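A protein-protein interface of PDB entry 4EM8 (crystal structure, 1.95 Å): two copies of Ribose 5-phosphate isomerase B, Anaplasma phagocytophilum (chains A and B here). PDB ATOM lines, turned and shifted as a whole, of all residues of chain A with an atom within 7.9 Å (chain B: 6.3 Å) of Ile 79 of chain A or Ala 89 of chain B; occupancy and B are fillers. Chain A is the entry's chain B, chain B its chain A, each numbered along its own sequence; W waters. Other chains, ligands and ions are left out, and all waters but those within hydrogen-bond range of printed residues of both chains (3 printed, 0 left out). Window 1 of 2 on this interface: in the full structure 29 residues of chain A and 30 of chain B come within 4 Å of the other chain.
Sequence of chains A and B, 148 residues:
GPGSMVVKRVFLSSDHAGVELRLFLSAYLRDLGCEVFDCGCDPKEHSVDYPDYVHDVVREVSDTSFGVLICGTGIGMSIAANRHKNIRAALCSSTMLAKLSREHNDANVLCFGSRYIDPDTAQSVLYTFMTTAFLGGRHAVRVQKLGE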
ATOM      1  N   TYR A  50     -21.433  -6.538  -2.098  1.00  0.00           N
ATOM      2  CA  TYR A  50     -21.067  -7.001  -3.447  1.00  0.00           C
ATOM      3  C   TYR A  50     -20.546  -5.914  -4.416  1.00  0.00           C
ATOM      4  O   TYR A  50     -19.630  -6.198  -5.205  1.00  0.00           O
ATOM      5  CB  TYR A  50     -22.175  -7.858  -4.080  1.00  0.00           C
ATOM      6  CG  TYR A  50     -23.509  -7.161  -4.215  1.00  0.00           C
ATOM      7  CD1 TYR A  50     -23.805  -6.401  -5.343  1.00  0.00           C
ATOM      8  CD2 TYR A  50     -24.486  -7.279  -3.223  1.00  0.00           C
ATOM      9  CE1 TYR A  50     -25.027  -5.738  -5.459  1.00  0.00           C
ATOM     10  CE2 TYR A  50     -25.701  -6.620  -3.338  1.00  0.00           C
ATOM     11  CZ  TYR A  50     -25.960  -5.851  -4.447  1.00  0.00           C
ATOM     12  OH  TYR A  50     -27.168  -5.218  -4.559  1.00  0.00           O
ATOM     13  N   VAL A  54     -16.639  -5.841  -7.600  1.00  0.00           N
ATOM     14  CA  VAL A  54     -16.789  -5.833  -9.057  1.00  0.00           C
ATOM     15  C   VAL A  54     -15.571  -5.259  -9.800  1.00  0.00           C
ATOM     16  O   VAL A  54     -15.113  -5.866 -10.762  1.00  0.00           O
ATOM     17  CB  VAL A  54     -18.052  -5.028  -9.445  1.00  0.00           C
ATOM     18  CG1 VAL A  54     -18.233  -5.012 -10.943  1.00  0.00           C
ATOM     19  CG2 VAL A  54     -19.276  -5.630  -8.764  1.00  0.00           C
ATOM     20  N   LEU A  69     -18.862 -13.430 -11.264  1.00  0.00           N
ATOM     21  CA  LEU A  69     -19.250 -12.657 -10.073  1.00  0.00           C
ATOM     22  C   LEU A  69     -20.362 -13.371  -9.341  1.00  0.00           C
ATOM     23  O   LEU A  69     -21.298 -13.846  -9.989  1.00  0.00           O
ATOM     24  CB  LEU A  69     -19.751 -11.294 -10.488  1.00  0.00           C
ATOM     25  CG  LEU A  69     -18.748 -10.345 -11.130  1.00  0.00           C
ATOM     26  CD1 LEU A  69     -19.499  -9.121 -11.627  1.00  0.00           C
ATOM     27  CD2 LEU A  69     -17.660  -9.989 -10.131  1.00  0.00           C
ATOM     28  N   CYS A  71     -22.959 -13.251  -5.886  1.00  0.00           N
ATOM     29  CA  CYS A  71     -23.599 -12.816  -4.656  1.00  0.00           C
ATOM     30  C   CYS A  71     -24.694 -13.832  -4.333  1.00  0.00           C
ATOM     31  O   CYS A  71     -24.815 -14.878  -4.984  1.00  0.00           O
ATOM     32  CB  CYS A  71     -24.145 -11.359  -4.737  1.00  0.00           C
ATOM     33  SG  CYS A  71     -25.438 -11.018  -5.982  1.00  0.00           S
ATOM     34  N   GLY A  74     -27.273 -13.205  -7.394  1.00  0.00           N
ATOM     35  CA  GLY A  74     -26.692 -12.873  -8.692  1.00  0.00           C
ATOM     36  C   GLY A  74     -27.164 -11.556  -9.286  1.00  0.00           C
ATOM     37  O   GLY A  74     -26.528 -11.029 -10.185  1.00  0.00           O
ATOM     38  N   ILE A  75     -28.286 -11.034  -8.784  1.00  0.00           N
ATOM     39  CA  ILE A  75     -28.964  -9.901  -9.377  1.00  0.00           C
ATOM     40  C   ILE A  75     -28.125  -8.653  -9.190  1.00  0.00           C
ATOM     41  O   ILE A  75     -27.925  -7.859 -10.117  1.00  0.00           O
ATOM     42  CB  ILE A  75     -30.345  -9.700  -8.721  1.00  0.00           C
ATOM     43  CG1 ILE A  75     -31.193 -10.979  -8.855  1.00  0.00           C
ATOM     44  CG2 ILE A  75     -31.069  -8.523  -9.343  1.00  0.00           C
ATOM     45  CD1 ILE A  75     -32.465 -10.961  -8.035  1.00  0.00           C
ATOM     46  N   GLY A  76     -27.629  -8.468  -7.981  1.00  0.00           N
ATOM     47  CA  GLY A  76     -26.812  -7.307  -7.676  1.00  0.00           C
ATOM     48  C   GLY A  76     -25.488  -7.296  -8.432  1.00  0.00           C
ATOM     49  O   GLY A  76     -25.043  -6.244  -8.925  1.00  0.00           O
ATOM     50  N   MET A  77     -24.856  -8.459  -8.521  1.00  0.00           N
ATOM     51  CA  MET A  77     -23.599  -8.565  -9.316  1.00  0.00           C
ATOM     52  C   MET A  77     -23.837  -8.230 -10.799  1.00  0.00           C
ATOM     53  O   MET A  77     -23.063  -7.505 -11.411  1.00  0.00           O
ATOM     54  CB  MET A  77     -22.955  -9.970  -9.174  1.00  0.00           C
ATOM     55  CG  MET A  77     -22.137 -10.213  -7.897  1.00  0.00           C
ATOM     56  SD  MET A  77     -20.938  -8.866  -7.607  1.00  0.00           S
ATOM     57  CE  MET A  77     -19.852  -9.724  -6.475  1.00  0.00           C
ATOM     58  N   SER A  78     -24.930  -8.722 -11.366  1.00  0.00           N
ATOM     59  CA  SER A  78     -25.199  -8.444 -12.780  1.00  0.00           C
ATOM     60  C   SER A  78     -25.523  -6.960 -13.026  1.00  0.00           C
ATOM     61  O   SER A  78     -25.017  -6.377 -13.999  1.00  0.00           O
ATOM     62  CB  SER A  78     -26.248  -9.397 -13.355  1.00  0.00           C
ATOM     63  OG  SER A  78     -27.427  -9.435 -12.579  1.00  0.00           O
ATOM     64  N   ILE A  79     -26.296  -6.326 -12.127  1.00  0.00           N
ATOM     65  CA  ILE A  79     -26.542  -4.881 -12.183  1.00  0.00           C
ATOM     66  C   ILE A  79     -25.221  -4.093 -12.148  1.00  0.00           C
ATOM     67  O   ILE A  79     -24.957  -3.303 -13.034  1.00  0.00           O
ATOM     68  CB  ILE A  79     -27.457  -4.378 -11.027  1.00  0.00           C
ATOM     69  CG1 ILE A  79     -28.871  -4.906 -11.176  1.00  0.00           C
ATOM     70  CG2 ILE A  79     -27.496  -2.850 -11.009  1.00  0.00           C
ATOM     71  CD1 ILE A  79     -29.752  -4.689  -9.950  1.00  0.00           C
ATOM     72  N   ALA A  80     -24.386  -4.377 -11.154  1.00  0.00           N
ATOM     73  CA  ALA A  80     -23.093  -3.714 -10.977  1.00  0.00           C
ATOM     74  C   ALA A  80     -22.127  -3.876 -12.161  1.00  0.00           C
ATOM     75  O   ALA A  80     -21.451  -2.913 -12.534  1.00  0.00           O
ATOM     76  CB  ALA A  80     -22.428  -4.213  -9.695  1.00  0.00           C
ATOM     77  N   ALA A  81     -22.023  -5.089 -12.698  1.00  0.00           N
ATOM     78  CA  ALA A  81     -21.060  -5.392 -13.754  1.00  0.00           C
ATOM     79  C   ALA A  81     -21.457  -4.642 -15.005  1.00  0.00           C
ATOM     80  O   ALA A  81     -20.586  -4.090 -15.714  1.00  0.00           O
ATOM     81  CB  ALA A  81     -21.002  -6.900 -14.033  1.00  0.00           C
ATOM     82  N   ASN A  82     -22.762  -4.534 -15.251  1.00  0.00           N
ATOM     83  CA  ASN A  82     -23.216  -3.962 -16.520  1.00  0.00           C
ATOM     84  C   ASN A  82     -23.212  -2.433 -16.546  1.00  0.00           C
ATOM     85  O   ASN A  82     -23.546  -1.834 -17.572  1.00  0.00           O
ATOM     86  CB  ASN A  82     -24.542  -4.550 -16.953  1.00  0.00           C
ATOM     87  CG  ASN A  82     -24.398  -5.972 -17.513  1.00  0.00           C
ATOM     88  OD1 ASN A  82     -23.500  -6.238 -18.315  1.00  0.00           O
ATOM     89  ND2 ASN A  82     -25.307  -6.892 -17.106  1.00  0.00           N
ATOM     90  N   ARG A  83     -22.819  -1.811 -15.433  1.00  0.00           N
ATOM     91  CA  ARG A  83     -22.467  -0.350 -15.424  1.00  0.00           C
ATOM     92  C   ARG A  83     -21.315   0.002 -16.382  1.00  0.00           C
ATOM     93  O   ARG A  83     -21.197   1.144 -16.798  1.00  0.00           O
ATOM     94  CB  ARG A  83     -22.088   0.109 -14.005  1.00  0.00           C
ATOM     95  CG  ARG A  83     -23.179  -0.030 -12.956  1.00  0.00           C
ATOM     96  CD  ARG A  83     -24.184   1.081 -13.060  1.00  0.00           C
ATOM     97  NE  ARG A  83     -25.151   1.118 -11.947  1.00  0.00           N
ATOM     98  CZ  ARG A  83     -26.398   0.656 -12.014  1.00  0.00           C
ATOM     99  NH1 ARG A  83     -26.848   0.077 -13.127  1.00  0.00           N
ATOM    100  NH2 ARG A  83     -27.195   0.766 -10.963  1.00  0.00           N
ATOM    101  N   HIS A  84     -20.511  -0.995 -16.750  1.00  0.00           N
ATOM    102  CA  HIS A  84     -19.298  -0.808 -17.548  1.00  0.00           C
ATOM    103  C   HIS A  84     -19.541  -1.222 -18.988  1.00  0.00           C
ATOM    104  O   HIS A  84     -19.985  -2.346 -19.281  1.00  0.00           O
ATOM    105  CB  HIS A  84     -18.167  -1.633 -16.921  1.00  0.00           C
ATOM    106  CG  HIS A  84     -17.919  -1.318 -15.461  1.00  0.00           C
ATOM    107  ND1 HIS A  84     -17.133  -0.305 -15.067  1.00  0.00           N
ATOM    108  CD2 HIS A  84     -18.423  -1.901 -14.291  1.00  0.00           C
ATOM    109  CE1 HIS A  84     -17.119  -0.251 -13.716  1.00  0.00           C
ATOM    110  NE2 HIS A  84     -17.901  -1.243 -13.248  1.00  0.00           N
ATOM    111  N   ALA A  89     -22.677  -8.869 -18.984  1.00  0.00           N
ATOM    112  CA  ALA A  89     -22.812  -9.788 -17.861  1.00  0.00           C
ATOM    113  C   ALA A  89     -24.194 -10.455 -17.871  1.00  0.00           C
ATOM    114  O   ALA A  89     -25.203  -9.810 -18.141  1.00  0.00           O
ATOM    115  CB  ALA A  89     -22.579  -9.009 -16.529  1.00  0.00           C
ATOM    116  N   LEU A  91     -26.701 -13.170 -15.556  1.00  0.00           N
ATOM    117  CA  LEU A  91     -27.001 -14.047 -14.450  1.00  0.00           C
ATOM    118  C   LEU A  91     -27.576 -15.314 -15.055  1.00  0.00           C
ATOM    119  O   LEU A  91     -28.656 -15.306 -15.628  1.00  0.00           O
ATOM    120  CB  LEU A  91     -28.024 -13.404 -13.518  1.00  0.00           C
ATOM    121  CG  LEU A  91     -28.649 -14.252 -12.399  1.00  0.00           C
ATOM    122  CD1 LEU A  91     -27.628 -15.059 -11.613  1.00  0.00           C
ATOM    123  CD2 LEU A  91     -29.480 -13.343 -11.486  1.00  0.00           C
ATOM    124  N   CYS A 111     -22.611 -14.214 -14.043  1.00  0.00           N
ATOM    125  CA  CYS A 111     -23.038 -13.975 -12.663  1.00  0.00           C
ATOM    126  C   CYS A 111     -23.839 -15.163 -12.132  1.00  0.00           C
ATOM    127  O   CYS A 111     -24.700 -15.710 -12.840  1.00  0.00           O
ATOM    128  CB  CYS A 111     -23.866 -12.706 -12.558  1.00  0.00           C
ATOM    129  SG  CYS A 111     -22.969 -11.226 -13.071  1.00  0.00           S
ATOM    130  N   LEU B  69     -38.603  -3.686 -20.114  1.00  0.00           N
ATOM    131  CA  LEU B  69     -37.892  -3.888 -21.390  1.00  0.00           C
ATOM    132  C   LEU B  69     -37.970  -5.321 -21.912  1.00  0.00           C
ATOM    133  O   LEU B  69     -37.778  -6.280 -21.150  1.00  0.00           O
ATOM    134  CB  LEU B  69     -36.430  -3.494 -21.204  1.00  0.00           C
ATOM    135  CG  LEU B  69     -36.159  -2.015 -20.848  1.00  0.00           C
ATOM    136  CD1 LEU B  69     -34.682  -1.845 -20.449  1.00  0.00           C
ATOM    137  CD2 LEU B  69     -36.490  -1.059 -21.993  1.00  0.00           C
ATOM    138  N   MET B  77     -31.500  -6.593 -23.188  1.00  0.00           N
ATOM    139  CA  MET B  77     -32.141  -5.457 -22.519  1.00  0.00           C
ATOM    140  C   MET B  77     -31.584  -5.228 -21.108  1.00  0.00           C
ATOM    141  O   MET B  77     -31.381  -4.089 -20.698  1.00  0.00           O
ATOM    142  CB  MET B  77     -33.658  -5.649 -22.445  1.00  0.00           C
ATOM    143  CG  MET B  77     -34.394  -5.410 -23.783  1.00  0.00           C
ATOM    144  SD  MET B  77     -34.073  -3.752 -24.403  1.00  0.00           S
ATOM    145  CE  MET B  77     -35.530  -3.507 -25.450  1.00  0.00           C
ATOM    146  N   SER B  78     -31.354  -6.297 -20.350  1.00  0.00           N
ATOM    147  CA  SER B  78     -30.824  -6.112 -18.970  1.00  0.00           C
ATOM    148  C   SER B  78     -29.418  -5.534 -18.958  1.00  0.00           C
ATOM    149  O   SER B  78     -29.114  -4.632 -18.176  1.00  0.00           O
ATOM    150  CB  SER B  78     -30.920  -7.388 -18.136  1.00  0.00           C
ATOM    151  OG  SER B  78     -30.355  -8.464 -18.840  1.00  0.00           O
ATOM    152  N   ILE B  79     -28.576  -5.985 -19.881  1.00  0.00           N
ATOM    153  CA  ILE B  79     -27.238  -5.414 -20.043  1.00  0.00           C
ATOM    154  C   ILE B  79     -27.325  -3.906 -20.371  1.00  0.00           C
ATOM    155  O   ILE B  79     -26.663  -3.087 -19.739  1.00  0.00           O
ATOM    156  CB  ILE B  79     -26.446  -6.125 -21.168  1.00  0.00           C
ATOM    157  CG1 ILE B  79     -26.082  -7.566 -20.775  1.00  0.00           C
ATOM    158  CG2 ILE B  79     -25.163  -5.359 -21.501  1.00  0.00           C
ATOM    159  CD1 ILE B  79     -25.621  -8.405 -21.969  1.00  0.00           C
ATOM    160  N   ALA B  81     -29.857  -1.748 -20.073  1.00  0.00           N
ATOM    161  CA  ALA B  81     -30.527  -1.002 -18.964  1.00  0.00           C
ATOM    162  C   ALA B  81     -29.576  -0.623 -17.861  1.00  0.00           C
ATOM    163  O   ALA B  81     -29.605   0.537 -17.373  1.00  0.00           O
ATOM    164  CB  ALA B  81     -31.663  -1.863 -18.337  1.00  0.00           C
ATOM    165  N   ASN B  82     -28.713  -1.582 -17.483  1.00  0.00           N
ATOM    166  CA  ASN B  82     -27.835  -1.412 -16.324  1.00  0.00           C
ATOM    167  C   ASN B  82     -26.572  -0.614 -16.590  1.00  0.00           C
ATOM    168  O   ASN B  82     -25.750  -0.420 -15.695  1.00  0.00           O
ATOM    169  CB  ASN B  82     -27.543  -2.754 -15.677  1.00  0.00           C
ATOM    170  CG  ASN B  82     -28.717  -3.230 -14.884  1.00  0.00           C
ATOM    171  OD1 ASN B  82     -29.350  -2.410 -14.213  1.00  0.00           O
ATOM    172  ND2 ASN B  82     -29.054  -4.530 -14.968  1.00  0.00           N
ATOM    173  N   ARG B  83     -26.442  -0.152 -17.821  1.00  0.00           N
ATOM    174  CA  ARG B  83     -25.456   0.881 -18.192  1.00  0.00           C
ATOM    175  C   ARG B  83     -25.666   2.200 -17.450  1.00  0.00           C
ATOM    176  O   ARG B  83     -24.716   2.961 -17.307  1.00  0.00           O
ATOM    177  CB  ARG B  83     -25.468   1.133 -19.722  1.00  0.00           C
ATOM    178  CG  ARG B  83     -25.024  -0.049 -20.567  1.00  0.00           C
ATOM    179  CD  ARG B  83     -23.529  -0.115 -20.694  1.00  0.00           C
ATOM    180  NE  ARG B  83     -23.072  -1.155 -21.626  1.00  0.00           N
ATOM    181  CZ  ARG B  83     -22.784  -2.430 -21.305  1.00  0.00           C
ATOM    182  NH1 ARG B  83     -22.918  -2.880 -20.061  1.00  0.00           N
ATOM    183  NH2 ARG B  83     -22.311  -3.263 -22.243  1.00  0.00           N
ATOM    184  N   ILE B  87     -30.588   3.067 -12.775  1.00  0.00           N
ATOM    185  CA  ILE B  87     -31.340   1.904 -13.177  1.00  0.00           C
ATOM    186  C   ILE B  87     -30.823   0.657 -12.505  1.00  0.00           C
ATOM    187  O   ILE B  87     -29.590   0.390 -12.444  1.00  0.00           O
ATOM    188  CB  ILE B  87     -31.266   1.676 -14.699  1.00  0.00           C
ATOM    189  CG1 ILE B  87     -31.819   2.876 -15.494  1.00  0.00           C
ATOM    190  CG2 ILE B  87     -32.016   0.404 -15.077  1.00  0.00           C
ATOM    191  CD1 ILE B  87     -33.265   3.285 -15.212  1.00  0.00           C
ATOM    192  N   ARG B  88     -31.782  -0.146 -12.037  1.00  0.00           N
ATOM    193  CA  ARG B  88     -31.486  -1.437 -11.441  1.00  0.00           C
ATOM    194  C   ARG B  88     -32.412  -2.436 -12.090  1.00  0.00           C
ATOM    195  O   ARG B  88     -33.567  -2.609 -11.647  1.00  0.00           O
ATOM    196  CB  ARG B  88     -31.662  -1.385  -9.913  1.00  0.00           C
ATOM    197  CG  ARG B  88     -30.693  -0.400  -9.262  1.00  0.00           C
ATOM    198  CD  ARG B  88     -30.880  -0.265  -7.759  1.00  0.00           C
ATOM    199  NE  ARG B  88     -32.203   0.246  -7.450  1.00  0.00           N
ATOM    200  CZ  ARG B  88     -32.549   1.529  -7.541  1.00  0.00           C
ATOM    201  NH1 ARG B  88     -31.654   2.434  -7.895  1.00  0.00           N
ATOM    202  NH2 ARG B  88     -33.785   1.908  -7.268  1.00  0.00           N
ATOM    203  N   ALA B  89     -31.911  -3.031 -13.189  1.00  0.00           N
ATOM    204  CA  ALA B  89     -32.688  -3.937 -14.029  1.00  0.00           C
ATOM    205  C   ALA B  89     -32.486  -5.396 -13.691  1.00  0.00           C
ATOM    206  O   ALA B  89     -31.378  -5.832 -13.455  1.00  0.00           O
ATOM    207  CB  ALA B  89     -32.369  -3.723 -15.511  1.00  0.00           C
ATOM    208  N   ALA B  90     -33.547  -6.184 -13.783  1.00  0.00           N
ATOM    209  CA  ALA B  90     -33.468  -7.645 -13.568  1.00  0.00           C
ATOM    210  C   ALA B  90     -34.300  -8.358 -14.631  1.00  0.00           C
ATOM    211  O   ALA B  90     -35.458  -8.023 -14.838  1.00  0.00           O
ATOM    212  CB  ALA B  90     -33.987  -8.010 -12.177  1.00  0.00           C
ATOM    213  N   LEU B  91     -33.686  -9.331 -15.306  1.00  0.00           N
ATOM    214  CA  LEU B  91     -34.398 -10.302 -16.153  1.00  0.00           C
ATOM    215  C   LEU B  91     -35.073 -11.335 -15.247  1.00  0.00           C
ATOM    216  O   LEU B  91     -34.397 -12.055 -14.505  1.00  0.00           O
ATOM    217  CB  LEU B  91     -33.410 -10.995 -17.103  1.00  0.00           C
ATOM    218  CG  LEU B  91     -33.881 -12.190 -17.943  1.00  0.00           C
ATOM    219  CD1 LEU B  91     -35.145 -11.816 -18.681  1.00  0.00           C
ATOM    220  CD2 LEU B  91     -32.763 -12.632 -18.900  1.00  0.00           C
ATOM    221  N   SER B 101     -35.581  -9.385  -6.577  1.00  0.00           N
ATOM    222  CA  SER B 101     -34.977  -8.187  -7.182  1.00  0.00           C
ATOM    223  C   SER B 101     -35.507  -6.884  -6.551  1.00  0.00           C
ATOM    224  O   SER B 101     -34.761  -5.885  -6.392  1.00  0.00           O
ATOM    225  CB  SER B 101     -35.175  -8.193  -8.720  1.00  0.00           C
ATOM    226  OG  SER B 101     -36.490  -7.772  -9.119  1.00  0.00           O
ATOM    227  N   ASN B 105     -32.693  -5.541  -4.219  1.00  0.00           N
ATOM    228  CA  ASN B 105     -32.017  -4.565  -5.074  1.00  0.00           C
ATOM    229  C   ASN B 105     -32.834  -3.319  -5.432  1.00  0.00           C
ATOM    230  O   ASN B 105     -32.339  -2.453  -6.190  1.00  0.00           O
ATOM    231  CB  ASN B 105     -31.499  -5.268  -6.328  1.00  0.00           C
ATOM    232  CG  ASN B 105     -30.829  -6.576  -5.998  1.00  0.00           C
ATOM    233  OD1 ASN B 105     -31.473  -7.624  -6.037  1.00  0.00           O
ATOM    234  ND2 ASN B 105     -29.540  -6.531  -5.646  1.00  0.00           N
ATOM    235  N   ALA B 107     -35.261  -3.121  -7.419  1.00  0.00           N
ATOM    236  CA  ALA B 107     -35.188  -3.126  -8.900  1.00  0.00           C
ATOM    237  C   ALA B 107     -36.270  -2.209  -9.456  1.00  0.00           C
ATOM    238  O   ALA B 107     -37.399  -2.224  -8.969  1.00  0.00           O
ATOM    239  CB  ALA B 107     -35.318  -4.536  -9.466  1.00  0.00           C
ATOM    240  N   ASN B 108     -35.908  -1.355 -10.420  1.00  0.00           N
ATOM    241  CA  ASN B 108     -36.869  -0.421 -11.000  1.00  0.00           C
ATOM    242  C   ASN B 108     -37.157  -0.670 -12.498  1.00  0.00           C
ATOM    243  O   ASN B 108     -38.026  -0.010 -13.072  1.00  0.00           O
ATOM    244  CB  ASN B 108     -36.473   1.035 -10.695  1.00  0.00           C
ATOM    245  CG  ASN B 108     -35.090   1.393 -11.171  1.00  0.00           C
ATOM    246  OD1 ASN B 108     -34.469   0.672 -11.977  1.00  0.00           O
ATOM    247  ND2 ASN B 108     -34.586   2.554 -10.696  1.00  0.00           N
ATOM    248  N   VAL B 109     -36.455  -1.632 -13.104  1.00  0.00           N
ATOM    249  CA  VAL B 109     -36.688  -2.091 -14.497  1.00  0.00           C
ATOM    250  C   VAL B 109     -36.757  -3.627 -14.572  1.00  0.00           C
ATOM    251  O   VAL B 109     -35.811  -4.361 -14.183  1.00  0.00           O
ATOM    252  CB  VAL B 109     -35.600  -1.566 -15.450  1.00  0.00           C
ATOM    253  CG1 VAL B 109     -35.686  -2.181 -16.864  1.00  0.00           C
ATOM    254  CG2 VAL B 109     -35.650  -0.034 -15.482  1.00  0.00           C
ATOM    255  N   LEU B 110     -37.886  -4.110 -15.075  1.00  0.00           N
ATOM    256  CA  LEU B 110     -38.123  -5.532 -15.279  1.00  0.00           C
ATOM    257  C   LEU B 110     -37.859  -5.897 -16.747  1.00  0.00           C
ATOM    258  O   LEU B 110     -38.441  -5.292 -17.653  1.00  0.00           O
ATOM    259  CB  LEU B 110     -39.548  -5.890 -14.855  1.00  0.00           C
ATOM    260  CG  LEU B 110     -40.133  -7.320 -15.077  1.00  0.00           C
ATOM    261  CD1 LEU B 110     -39.226  -8.410 -14.518  1.00  0.00           C
ATOM    262  CD2 LEU B 110     -41.548  -7.438 -14.492  1.00  0.00           C
ATOM    263  N   CYS B 111     -36.968  -6.860 -16.986  1.00  0.00           N
ATOM    264  CA  CYS B 111     -36.717  -7.355 -18.339  1.00  0.00           C
ATOM    265  C   CYS B 111     -37.325  -8.743 -18.579  1.00  0.00           C
ATOM    266  O   CYS B 111     -37.222  -9.584 -17.721  1.00  0.00           O
ATOM    267  CB  CYS B 111     -35.210  -7.417 -18.579  1.00  0.00           C
ATOM    268  SG  CYS B 111     -34.413  -5.799 -18.373  1.00  0.00           S
ATOM    269  N   LEU B 146     -24.697   0.870  -5.742  1.00  0.00           N
ATOM    270  CA  LEU B 146     -25.032   0.602  -7.150  1.00  0.00           C
ATOM    271  C   LEU B 146     -25.226   1.873  -7.973  1.00  0.00           C
ATOM    272  O   LEU B 146     -25.063   1.848  -9.185  1.00  0.00           O
ATOM    273  CB  LEU B 146     -26.278  -0.292  -7.277  1.00  0.00           C
ATOM    274  CG  LEU B 146     -26.190  -1.769  -6.895  1.00  0.00           C
ATOM    275  CD1 LEU B 146     -27.530  -2.501  -7.099  1.00  0.00           C
ATOM    276  CD2 LEU B 146     -25.087  -2.436  -7.706  1.00  0.00           C
HETATM  277  O   HOH W   1     -28.703   2.379  -8.782  1.00  0.00           O
HETATM  278  O   HOH W   2     -28.083  -9.151  -4.961  1.00  0.00           O
HETATM  279  O   HOH W   3     -27.839  -7.114 -15.892  1.00  0.00           O
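Tyr 50 of chain A touches Leu 146 of chain B (OH to CD1, 3.7 Å). CD1 of Ile 75 of chain A touches N of Ser 101 of chain B, at 3.8 Å. Ile 75 of chain A touches Asn 105 of chain B. ND2 of Asn 105 of chain B touches CA of Gly 76 of chain A (3.5 Å). Leu 146 of chain B touches Gly 76 of chain A. Ile 79 of chain A touches Arg 88 of chain B (CD1 to CB, 3.8 Å). O of Ala 89 of chain B touches CG1 of Ile 79 of chain A, 3.5 Å away. Leu 146 of chain B touches Ala 80 of chain A. Asn 82 of chain A touches Ile 79 of chain B (OD1 to CG2, 3.7 Å). Arg 83 of chain A touches Arg 83 of chain B (O to O, 3.99 Å).
O of Ser 78 of chain B lies within hydrogen-bond range of ND2 of Asn 82 of chain B (3.2 Å). The backbone NH (N) of Ala 89 of chain B is in hydrogen-bond range of the side-chain amide oxygen (OD1) of Asn 82 of chain B (2.8 Å). The guanidinium group (NE) of Arg 88 of chain B is in hydrogen-bond range of the backbone carbonyl oxygen (O) of Asn 105 of chain B (3.0 Å). The backbone NH (N) of Arg 88 of chain B sits at hydrogen-bond distance from the side-chain amide oxygen (OD1) of Asn 108 of chain B, at 2.8 Å. The backbone carbonyl oxygen (O) of Arg 88 of chain B is in hydrogen-bond range of the backbone NH (N) of Val 109 of chain B, 3.4 Å away. The side-chain hydroxyl (OG) of Ser 78 of chain A lies within hydrogen-bond range of the backbone carbonyl oxygen (O) of Ile 75 of chain A, at 3.0 Å.
Water W3 lies within hydrogen-bond range of ND2 of Asn 82 of chain A (2.8 Å), ND2 of Asn 82 of chain B (3.0 Å) and O of Ser 78 of chain A (3.5 Å). Water W2 lies within hydrogen-bond range of ND2 of Asn 105 of chain B (3.1 Å), N of Gly 76 of chain A (3.1 Å) and SG of Cys 71 of chain A (3.4 Å). Water W1 bridges the guanidinium group of Arg 88 of chain B and the guanidinium group of Arg 83 of chain A.
NH1 of Arg 83 of chain A sits at hydrogen-bond distance from O of Asn 82 of chain B, at 2.8 Å. The guanidinium group (NH1) of Arg 83 of chain B lies within hydrogen-bond range of the backbone carbonyl oxygen (O) of Asn 82 of chain A (2.8 Å). NH1 of Arg 83 of chain B sits at hydrogen-bond distance from O of His 84 of chain A, at 3.1 Å. O of Ile 87 of chain B sits at hydrogen-bond distance from NH2 of Arg 83 of chain A, at 2.8 Å. ND2 of Asn 105 of chain B lies within hydrogen-bond range of OH of Tyr 50 of chain A, at 2.9 Å. The backbone carbonyl oxygen of Leu 146 of chain B lies within hydrogen-bond range of the guanidinium group of Arg 83 of chain A (2.9 Å). The backbone carbonyl oxygen (O) of Asn 82 of chain A sits close to the backbone carbonyl oxygen (O) of Asn 82 of chain B, at 3.2 Å.
Of the 20 printed residues of chain B, 9 touch a printed residue of chain A. Hydrophobic or aromatic side chains of chain B within 4 Å of the printed part of chain A: Ile 79 and Leu 146. Of the 18 printed residues of chain A, 9 touch a printed residue of chain B. Hydrophobic or aromatic side chains of chain A that line the printed part of chain B: Tyr 50, Ile 75, Ile 79 and Ala 80. Among the printed residues, 20 pairs touch across the chains.
Ile 79 of chain A touches Ala 89 of chain B, and with the chains exchanged Ala 89 of chain A touches Ile 79 of chain B. Asn 82 of chain A touches its own counterpart, Asn 82 of chain B. Asn 82 of chain A touches Arg 83 of chain B, and with the chains exchanged Arg 83 of chain A touches Asn 82 of chain B. Arg 83 of chain B touches its own counterpart, Arg 83 of chain A. 10 positions are printed for both chains. Of the 20 pairs that touch across the chains among the printed residues, 8 have their exchanged pair printed and touching as well.
Ile 79 of chain A touches four residues of chain B. Ala 89 of chain B touches just one residue of chain A: Ile 79 (3.5 Å). Of the printed residues of chain B, Ala 80 of chain A touches Leu 146 (3.8 Å). Of the printed residues of chain A, Ile 87 of chain B touches Arg 83. Of the printed residues of chain B, Ala 89 of chain A touches Ile 79 (3.6 Å). Printed residues of chain B within 4 Å of Tyr 50 of chain A: Asn 105 and Leu 146. Cys 71 of chain A touches none of the printed residues of chain B. Ala 107 of chain B touches none of the printed residues of chain A. The nearest printed residue of chain B that does not touch Arg 83 of chain A is Arg 88 of chain B (4.1 Å).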
